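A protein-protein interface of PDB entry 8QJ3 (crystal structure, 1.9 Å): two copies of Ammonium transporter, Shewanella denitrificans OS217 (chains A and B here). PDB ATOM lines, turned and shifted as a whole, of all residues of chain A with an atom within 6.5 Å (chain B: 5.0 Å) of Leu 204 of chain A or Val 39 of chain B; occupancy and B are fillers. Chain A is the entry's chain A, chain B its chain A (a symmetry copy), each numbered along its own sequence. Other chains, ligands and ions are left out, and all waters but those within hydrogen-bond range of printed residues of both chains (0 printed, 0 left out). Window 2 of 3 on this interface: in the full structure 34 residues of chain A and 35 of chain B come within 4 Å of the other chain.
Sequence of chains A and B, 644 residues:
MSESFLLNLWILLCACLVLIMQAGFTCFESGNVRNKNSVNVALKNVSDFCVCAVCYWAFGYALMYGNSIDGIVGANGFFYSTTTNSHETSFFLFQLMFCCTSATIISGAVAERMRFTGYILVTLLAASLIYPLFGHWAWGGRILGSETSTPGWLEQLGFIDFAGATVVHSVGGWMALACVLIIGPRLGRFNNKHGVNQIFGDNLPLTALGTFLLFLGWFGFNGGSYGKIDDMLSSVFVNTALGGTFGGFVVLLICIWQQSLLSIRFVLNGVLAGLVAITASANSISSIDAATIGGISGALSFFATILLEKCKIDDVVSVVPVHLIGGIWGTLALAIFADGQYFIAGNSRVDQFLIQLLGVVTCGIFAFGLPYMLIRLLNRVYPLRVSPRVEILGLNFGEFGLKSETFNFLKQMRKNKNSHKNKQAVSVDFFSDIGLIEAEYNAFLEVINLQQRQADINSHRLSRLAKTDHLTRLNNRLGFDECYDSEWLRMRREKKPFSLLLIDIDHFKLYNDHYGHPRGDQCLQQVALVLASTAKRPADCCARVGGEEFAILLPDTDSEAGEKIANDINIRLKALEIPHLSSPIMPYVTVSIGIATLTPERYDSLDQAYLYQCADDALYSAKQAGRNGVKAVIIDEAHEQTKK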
ATOM      1  N   CYS A  27      16.447  23.320   4.048  1.00  0.00           N
ATOM      2  CA  CYS A  27      16.084  21.901   4.167  1.00  0.00           C
ATOM      3  C   CYS A  27      16.582  21.094   2.967  1.00  0.00           C
ATOM      4  O   CYS A  27      17.116  20.021   3.143  1.00  0.00           O
ATOM      5  CB  CYS A  27      14.562  21.751   4.262  1.00  0.00           C
ATOM      6  SG  CYS A  27      13.887  22.423   5.812  1.00  0.00           S
ATOM      7  N   SER A  30      20.390  20.924   3.180  1.00  0.00           N
ATOM      8  CA  SER A  30      20.952  20.256   4.348  1.00  0.00           C
ATOM      9  C   SER A  30      20.699  18.761   4.276  1.00  0.00           C
ATOM     10  O   SER A  30      21.544  17.932   4.569  1.00  0.00           O
ATOM     11  CB  SER A  30      20.466  20.982   5.664  1.00  0.00           C
ATOM     12  OG  SER A  30      19.469  20.219   6.114  1.00  0.00           O
ATOM     13  N   GLY A  31      19.592  18.325   3.716  1.00  0.00           N
ATOM     14  CA  GLY A  31      19.366  16.935   3.521  1.00  0.00           C
ATOM     15  C   GLY A  31      20.198  16.248   2.427  1.00  0.00           C
ATOM     16  O   GLY A  31      20.244  15.022   2.390  1.00  0.00           O
ATOM     17  N   ASN A  32      20.780  17.026   1.515  1.00  0.00           N
ATOM     18  CA  ASN A  32      21.573  16.488   0.436  1.00  0.00           C
ATOM     19  C   ASN A  32      23.043  16.439   0.839  1.00  0.00           C
ATOM     20  O   ASN A  32      23.875  16.043   0.049  1.00  0.00           O
ATOM     21  CB  ASN A  32      21.390  17.341  -0.801  1.00  0.00           C
ATOM     22  CG  ASN A  32      20.175  16.886  -1.580  1.00  0.00           C
ATOM     23  OD1 ASN A  32      20.016  15.702  -1.834  1.00  0.00           O
ATOM     24  ND2 ASN A  32      19.268  17.772  -1.870  1.00  0.00           N
ATOM     25  N   VAL A  33      23.362  16.801   2.088  1.00  0.00           N
ATOM     26  CA  VAL A  33      24.746  16.753   2.498  1.00  0.00           C
ATOM     27  C   VAL A  33      24.911  15.772   3.651  1.00  0.00           C
ATOM     28  O   VAL A  33      23.968  15.427   4.388  1.00  0.00           O
ATOM     29  CB  VAL A  33      25.368  18.129   2.806  1.00  0.00           C
ATOM     30  CG1 VAL A  33      25.158  19.203   1.758  1.00  0.00           C
ATOM     31  CG2 VAL A  33      25.023  18.623   4.178  1.00  0.00           C
ATOM     32  N   PHE A 200      25.663  10.628  -1.068  1.00  0.00           N
ATOM     33  CA  PHE A 200      24.240  10.791  -0.788  1.00  0.00           C
ATOM     34  C   PHE A 200      24.139  11.598   0.485  1.00  0.00           C
ATOM     35  O   PHE A 200      24.932  11.381   1.372  1.00  0.00           O
ATOM     36  CB  PHE A 200      23.525   9.454  -0.519  1.00  0.00           C
ATOM     37  CG  PHE A 200      23.670   8.451  -1.630  1.00  0.00           C
ATOM     38  CD1 PHE A 200      23.062   8.671  -2.863  1.00  0.00           C
ATOM     39  CD2 PHE A 200      24.391   7.290  -1.450  1.00  0.00           C
ATOM     40  CE1 PHE A 200      23.183   7.752  -3.901  1.00  0.00           C
ATOM     41  CE2 PHE A 200      24.524   6.377  -2.487  1.00  0.00           C
ATOM     42  CZ  PHE A 200      23.922   6.607  -3.713  1.00  0.00           C
ATOM     43  N   GLY A 201      23.138  12.468   0.554  1.00  0.00           N
ATOM     44  CA  GLY A 201      22.828  13.188   1.777  1.00  0.00           C
ATOM     45  C   GLY A 201      22.409  12.265   2.906  1.00  0.00           C
ATOM     46  O   GLY A 201      21.992  11.124   2.690  1.00  0.00           O
ATOM     47  N   ASP A 202      22.574  12.742   4.128  1.00  0.00           N
ATOM     48  CA  ASP A 202      22.140  11.986   5.292  1.00  0.00           C
ATOM     49  C   ASP A 202      20.774  12.448   5.790  1.00  0.00           C
ATOM     50  O   ASP A 202      20.325  11.934   6.776  1.00  0.00           O
ATOM     51  CB  ASP A 202      23.137  12.075   6.429  1.00  0.00           C
ATOM     52  CG  ASP A 202      24.414  11.303   6.097  1.00  0.00           C
ATOM     53  OD1 ASP A 202      24.307  10.271   5.381  1.00  0.00           O
ATOM     54  OD2 ASP A 202      25.507  11.684   6.587  1.00  0.00           O
ATOM     55  N   ASN A 203      20.067  13.398   5.170  1.00  0.00           N
ATOM     56  CA  ASN A 203      18.736  13.599   5.750  1.00  0.00           C
ATOM     57  C   ASN A 203      17.716  13.906   4.670  1.00  0.00           C
ATOM     58  O   ASN A 203      17.107  15.005   4.601  1.00  0.00           O
ATOM     59  CB  ASN A 203      18.748  14.743   6.752  1.00  0.00           C
ATOM     60  CG  ASN A 203      17.462  14.814   7.543  1.00  0.00           C
ATOM     61  OD1 ASN A 203      16.489  14.119   7.259  1.00  0.00           O
ATOM     62  ND2 ASN A 203      17.459  15.657   8.562  1.00  0.00           N
ATOM     63  N   LEU A 204      17.527  12.904   3.831  1.00  0.00           N
ATOM     64  CA  LEU A 204      16.815  13.166   2.585  1.00  0.00           C
ATOM     65  C   LEU A 204      15.350  13.453   2.874  1.00  0.00           C
ATOM     66  O   LEU A 204      14.739  14.122   2.075  1.00  0.00           O
ATOM     67  CB  LEU A 204      17.003  12.033   1.549  1.00  0.00           C
ATOM     68  CG  LEU A 204      18.453  11.854   1.058  1.00  0.00           C
ATOM     69  CD1 LEU A 204      18.625  10.519   0.309  1.00  0.00           C
ATOM     70  CD2 LEU A 204      18.851  13.021   0.150  1.00  0.00           C
ATOM     71  N   PRO A 205      14.713  13.028   3.958  1.00  0.00           N
ATOM     72  CA  PRO A 205      13.337  13.484   4.228  1.00  0.00           C
ATOM     73  C   PRO A 205      13.233  14.978   4.327  1.00  0.00           C
ATOM     74  O   PRO A 205      12.224  15.556   3.970  1.00  0.00           O
ATOM     75  CB  PRO A 205      12.939  12.944   5.601  1.00  0.00           C
ATOM     76  CG  PRO A 205      13.926  11.829   5.796  1.00  0.00           C
ATOM     77  CD  PRO A 205      15.178  12.101   4.981  1.00  0.00           C
ATOM     78  N   LEU A 206      14.301  15.609   4.832  1.00  0.00           N
ATOM     79  CA  LEU A 206      14.306  17.063   4.882  1.00  0.00           C
ATOM     80  C   LEU A 206      14.308  17.662   3.487  1.00  0.00           C
ATOM     81  O   LEU A 206      13.778  18.737   3.248  1.00  0.00           O
ATOM     82  CB  LEU A 206      15.525  17.496   5.710  1.00  0.00           C
ATOM     83  CG  LEU A 206      15.326  18.649   6.686  1.00  0.00           C
ATOM     84  CD1 LEU A 206      14.184  18.383   7.615  1.00  0.00           C
ATOM     85  CD2 LEU A 206      16.669  18.955   7.401  1.00  0.00           C
ATOM     86  N   THR A 207      14.845  16.941   2.509  1.00  0.00           N
ATOM     87  CA  THR A 207      14.802  17.474   1.161  1.00  0.00           C
ATOM     88  C   THR A 207      13.419  17.431   0.545  1.00  0.00           C
ATOM     89  O   THR A 207      13.077  18.327  -0.222  1.00  0.00           O
ATOM     90  CB  THR A 207      15.827  16.830   0.208  1.00  0.00           C
ATOM     91  OG1 THR A 207      15.356  15.513  -0.041  1.00  0.00           O
ATOM     92  CG2 THR A 207      17.186  16.836   0.822  1.00  0.00           C
ATOM     93  N   ALA A 208      12.565  16.513   0.942  1.00  0.00           N
ATOM     94  CA  ALA A 208      11.203  16.544   0.511  1.00  0.00           C
ATOM     95  C   ALA A 208      10.427  17.672   1.196  1.00  0.00           C
ATOM     96  O   ALA A 208       9.584  18.346   0.551  1.00  0.00           O
ATOM     97  CB  ALA A 208      10.611  15.211   0.780  1.00  0.00           C
ATOM     98  N   LEU A 209      10.635  17.826   2.532  1.00  0.00           N
ATOM     99  CA  LEU A 209      10.057  18.976   3.229  1.00  0.00           C
ATOM    100  C   LEU A 209      10.442  20.234   2.472  1.00  0.00           C
ATOM    101  O   LEU A 209       9.636  21.105   2.160  1.00  0.00           O
ATOM    102  CB  LEU A 209      10.583  19.087   4.672  1.00  0.00           C
ATOM    103  CG  LEU A 209      10.218  20.381   5.430  1.00  0.00           C
ATOM    104  CD1 LEU A 209       8.691  20.571   5.497  1.00  0.00           C
ATOM    105  CD2 LEU A 209      10.761  20.251   6.834  1.00  0.00           C
ATOM    106  N   LEU A 262      18.478   6.041  -6.089  1.00  0.00           N
ATOM    107  CA  LEU A 262      18.086   7.259  -5.376  1.00  0.00           C
ATOM    108  C   LEU A 262      17.278   8.208  -6.291  1.00  0.00           C
ATOM    109  O   LEU A 262      17.645   9.383  -6.514  1.00  0.00           O
ATOM    110  CB  LEU A 262      19.339   7.907  -4.755  1.00  0.00           C
ATOM    111  CG  LEU A 262      19.235   8.191  -3.246  1.00  0.00           C
ATOM    112  CD1 LEU A 262      19.694   6.992  -2.410  1.00  0.00           C
ATOM    113  CD2 LEU A 262      20.006   9.448  -2.852  1.00  0.00           C
ATOM    114  N   ILE A 264      14.790   9.736  -5.709  1.00  0.00           N
ATOM    115  CA  ILE A 264      14.109  10.773  -4.948  1.00  0.00           C
ATOM    116  C   ILE A 264      14.849  12.054  -5.322  1.00  0.00           C
ATOM    117  O   ILE A 264      14.261  13.110  -5.649  1.00  0.00           O
ATOM    118  CB  ILE A 264      14.030  10.475  -3.440  1.00  0.00           C
ATOM    119  CG1 ILE A 264      13.213  11.557  -2.730  1.00  0.00           C
ATOM    120  CG2 ILE A 264      15.440  10.311  -2.868  1.00  0.00           C
ATOM    121  CD1 ILE A 264      13.211  11.450  -1.207  1.00  0.00           C
ATOM    122  N   ARG A 265      16.164  11.924  -5.419  1.00  0.00           N
ATOM    123  CA  ARG A 265      16.835  13.158  -5.775  1.00  0.00           C
ATOM    124  C   ARG A 265      16.265  13.668  -7.109  1.00  0.00           C
ATOM    125  O   ARG A 265      16.171  14.938  -7.263  1.00  0.00           O
ATOM    126  CB  ARG A 265      18.346  12.969  -5.693  1.00  0.00           C
ATOM    127  CG  ARG A 265      18.801  12.524  -4.298  1.00  0.00           C
ATOM    128  CD  ARG A 265      20.290  12.702  -4.095  1.00  0.00           C
ATOM    129  NE  ARG A 265      21.098  12.203  -5.214  1.00  0.00           N
ATOM    130  CZ  ARG A 265      22.440  12.165  -5.226  1.00  0.00           C
ATOM    131  NH1 ARG A 265      23.120  12.636  -4.191  1.00  0.00           N
ATOM    132  NH2 ARG A 265      23.094  11.628  -6.258  1.00  0.00           N
ATOM    133  N   LEU A 268      12.447  15.152  -7.148  1.00  0.00           N
ATOM    134  CA  LEU A 268      12.356  16.395  -6.398  1.00  0.00           C
ATOM    135  C   LEU A 268      12.912  17.562  -7.221  1.00  0.00           C
ATOM    136  O   LEU A 268      12.315  18.635  -7.276  1.00  0.00           O
ATOM    137  CB  LEU A 268      13.095  16.221  -5.071  1.00  0.00           C
ATOM    138  CG  LEU A 268      12.254  15.569  -3.972  1.00  0.00           C
ATOM    139  CD1 LEU A 268      11.657  14.263  -4.464  1.00  0.00           C
ATOM    140  CD2 LEU A 268      13.059  15.365  -2.706  1.00  0.00           C
ATOM    141  N   ASN B  35      14.981   5.020  10.467  1.00  0.00           N
ATOM    142  CA  ASN B  35      15.950   5.627   9.573  1.00  0.00           C
ATOM    143  C   ASN B  35      16.177   4.819   8.281  1.00  0.00           C
ATOM    144  O   ASN B  35      16.335   5.416   7.202  1.00  0.00           O
ATOM    145  CB  ASN B  35      17.302   5.786  10.246  1.00  0.00           C
ATOM    146  CG  ASN B  35      17.382   6.965  11.198  1.00  0.00           C
ATOM    147  OD1 ASN B  35      16.748   7.999  10.972  1.00  0.00           O
ATOM    148  ND2 ASN B  35      18.166   6.805  12.255  1.00  0.00           N
ATOM    149  N   ASN B  37      14.219   3.352   6.501  1.00  0.00           N
ATOM    150  CA  ASN B  37      13.091   3.548   5.613  1.00  0.00           C
ATOM    151  C   ASN B  37      12.803   5.027   5.260  1.00  0.00           C
ATOM    152  O   ASN B  37      11.856   5.283   4.483  1.00  0.00           O
ATOM    153  CB  ASN B  37      11.804   2.984   6.193  1.00  0.00           C
ATOM    154  CG  ASN B  37      11.846   1.456   6.292  1.00  0.00           C
ATOM    155  OD1 ASN B  37      12.252   0.823   5.331  1.00  0.00           O
ATOM    156  ND2 ASN B  37      11.553   0.870   7.445  1.00  0.00           N
ATOM    157  N   SER B  38      13.696   5.935   5.728  1.00  0.00           N
ATOM    158  CA  SER B  38      13.430   7.385   5.812  1.00  0.00           C
ATOM    159  C   SER B  38      13.249   8.000   4.409  1.00  0.00           C
ATOM    160  O   SER B  38      12.296   8.769   4.171  1.00  0.00           O
ATOM    161  CB  SER B  38      14.502   8.088   6.640  1.00  0.00           C
ATOM    162  OG  SER B  38      15.819   7.967   6.035  1.00  0.00           O
ATOM    163  N   VAL B  39      14.051   7.543   3.463  1.00  0.00           N
ATOM    164  CA  VAL B  39      14.025   8.116   2.136  1.00  0.00           C
ATOM    165  C   VAL B  39      12.767   7.728   1.353  1.00  0.00           C
ATOM    166  O   VAL B  39      12.298   8.500   0.507  1.00  0.00           O
ATOM    167  CB  VAL B  39      15.318   7.730   1.430  1.00  0.00           C
ATOM    168  CG1 VAL B  39      15.417   8.353   0.052  1.00  0.00           C
ATOM    169  CG2 VAL B  39      16.481   8.132   2.341  1.00  0.00           C
ATOM    170  N   ASN B  40      12.245   6.533   1.628  1.00  0.00           N
ATOM    171  CA  ASN B  40      11.112   6.002   0.892  1.00  0.00           C
ATOM    172  C   ASN B  40       9.904   6.879   1.105  1.00  0.00           C
ATOM    173  O   ASN B  40       9.179   7.304   0.199  1.00  0.00           O
ATOM    174  CB  ASN B  40      10.785   4.574   1.300  1.00  0.00           C
ATOM    175  CG  ASN B  40       9.637   4.056   0.440  1.00  0.00           C
ATOM    176  OD1 ASN B  40       9.844   3.734  -0.724  1.00  0.00           O
ATOM    177  ND2 ASN B  40       8.442   4.144   0.972  1.00  0.00           N
ATOM    178  N   VAL B  41       9.783   7.364   2.318  1.00  0.00           N
ATOM    179  CA  VAL B  41       8.583   8.066   2.667  1.00  0.00           C
ATOM    180  C   VAL B  41       8.534   9.396   1.959  1.00  0.00           C
ATOM    181  O   VAL B  41       7.524   9.802   1.364  1.00  0.00           O
ATOM    182  CB  VAL B  41       8.465   8.092   4.195  1.00  0.00           C
ATOM    183  CG1 VAL B  41       7.580   9.306   4.531  1.00  0.00           C
ATOM    184  CG2 VAL B  41       8.044   6.627   4.668  1.00  0.00           C
ATOM    185  N   ALA B  42       9.690   9.982   1.811  1.00  0.00           N
ATOM    186  CA  ALA B  42       9.841  11.205   1.098  1.00  0.00           C
ATOM    187  C   ALA B  42       9.591  11.095  -0.405  1.00  0.00           C
ATOM    188  O   ALA B  42       9.080  12.047  -1.062  1.00  0.00           O
ATOM    189  CB  ALA B  42      11.261  11.626   1.311  1.00  0.00           C
ATOM    190  N   LEU B  43      10.179  10.033  -1.000  1.00  0.00           N
ATOM    191  CA  LEU B  43       9.979   9.824  -2.416  1.00  0.00           C
ATOM    192  C   LEU B  43       8.495   9.613  -2.723  1.00  0.00           C
ATOM    193  O   LEU B  43       8.030  10.124  -3.706  1.00  0.00           O
ATOM    194  CB  LEU B  43      10.763   8.579  -2.850  1.00  0.00           C
ATOM    195  CG  LEU B  43      10.465   8.170  -4.284  1.00  0.00           C
ATOM    196  CD1 LEU B  43      10.985   9.200  -5.280  1.00  0.00           C
ATOM    197  CD2 LEU B  43      11.051   6.788  -4.551  1.00  0.00           C
ATOM    198  N   ASN B 396      15.311   2.149   2.062  1.00  0.00           N
ATOM    199  CA  ASN B 396      16.398   2.963   1.545  1.00  0.00           C
ATOM    200  C   ASN B 396      17.464   2.188   0.765  1.00  0.00           C
ATOM    201  O   ASN B 396      17.760   2.607  -0.343  1.00  0.00           O
ATOM    202  CB  ASN B 396      17.242   3.693   2.580  1.00  0.00           C
ATOM    203  CG  ASN B 396      16.436   4.674   3.393  1.00  0.00           C
ATOM    204  OD1 ASN B 396      15.233   4.825   3.214  1.00  0.00           O
ATOM    205  ND2 ASN B 396      17.111   5.278   4.346  1.00  0.00           N
ATOM    206  N   PHE B 400      16.043   1.447  -2.838  1.00  0.00           N
ATOM    207  CA  PHE B 400      16.522   2.643  -3.541  1.00  0.00           C
ATOM    208  C   PHE B 400      18.054   2.705  -3.619  1.00  0.00           C
ATOM    209  O   PHE B 400      18.519   3.688  -4.153  1.00  0.00           O
ATOM    210  CB  PHE B 400      16.042   3.924  -2.878  1.00  0.00           C
ATOM    211  CG  PHE B 400      14.544   4.025  -2.797  1.00  0.00           C
ATOM    212  CD1 PHE B 400      13.793   4.296  -3.928  1.00  0.00           C
ATOM    213  CD2 PHE B 400      13.879   3.760  -1.617  1.00  0.00           C
ATOM    214  CE1 PHE B 400      12.418   4.354  -3.860  1.00  0.00           C
ATOM    215  CE2 PHE B 400      12.511   3.802  -1.562  1.00  0.00           C
ATOM    216  CZ  PHE B 400      11.787   4.129  -2.664  1.00  0.00           C
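N of Leu 262 of chain A is in hydrogen-bond range of O of Phe 400 of chain B (3.0 Å).
The backbone carbonyl oxygen (O) of Leu 204 of chain A lies within hydrogen-bond range of the side-chain hydroxyl (OG1) of Thr 207 of chain A (2.6 Å). The backbone carbonyl oxygen (O) of Asn 35 of chain B lies within hydrogen-bond range of the side-chain hydroxyl (OG) of Ser 38 of chain B (2.9 Å). The side-chain amide oxygen of Asn 396 of chain B sits at hydrogen-bond distance from the backbone NH of Ser 38 of chain B, 3.1 Å away. The backbone NH (N) of Val 39 of chain B is in hydrogen-bond range of the side-chain amide oxygen (OD1) of Asn 396 of chain B (3.0 Å).
Val 39 of chain B touches Leu 204 of chain A (CG2 to CD1, 3.8 Å). CG of Pro 205 of chain A touches O of Ser 38 of chain B, at 3.8 Å. Ala 208 of chain A touches Ala 42 of chain B (CB to CB, 3.7 Å). Val 39 of chain B touches Ile 264 of chain A. CD1 of Ile 264 of chain A touches CB of Ala 42 of chain B (3.2 Å). Leu 43 of chain B touches Ile 264 of chain A.
Of the printed residues of chain B, Leu 204 of chain A touches Val 39. Of the printed residues of chain B, Pro 205 of chain A touches Ser 38 (3.8 Å). Of the printed residues of chain B, Leu 262 of chain A touches Phe 400 (3.0 Å). Printed residues of chain B within 4 Å of Ile 264 of chain A: Val 39 (3.5 Å), Ala 42 (3.2 Å) and Leu 43 (3.4 Å). Of the printed residues of chain A, Val 39 of chain B touches Leu 204 (3.8 Å) and Ile 264 (3.5 Å). Of the printed residues of chain A, Ala 42 of chain B touches Ala 208 (3.7 Å) and Ile 264 (3.2 Å). The nearest printed residue of chain A that does not touch Val 39 of chain B is Pro 205 of chain A (4.9 Å). The nearest printed residue of chain A that does not touch Ala 42 of chain B is Pro 205 of chain A (4.03 Å).
Hydrophobic or aromatic side chains of chain B that line the printed part of chain A: Val 39, Ala 42 and Leu 43. Of the 19 printed residues of chain A, 5 touch a printed residue of chain B. Hydrophobic or aromatic side chains of chain A that line the printed part of chain B: Leu 204, Pro 205, Ala 208, Leu 262 and Ile 264. Among the printed residues, 7 pairs touch across the chains. Among the printed residues, no Asp or Glu carboxylate lies within 4 Å of a Lys or Arg side-chain nitrogen of the other chain.
No position is printed for both chains.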
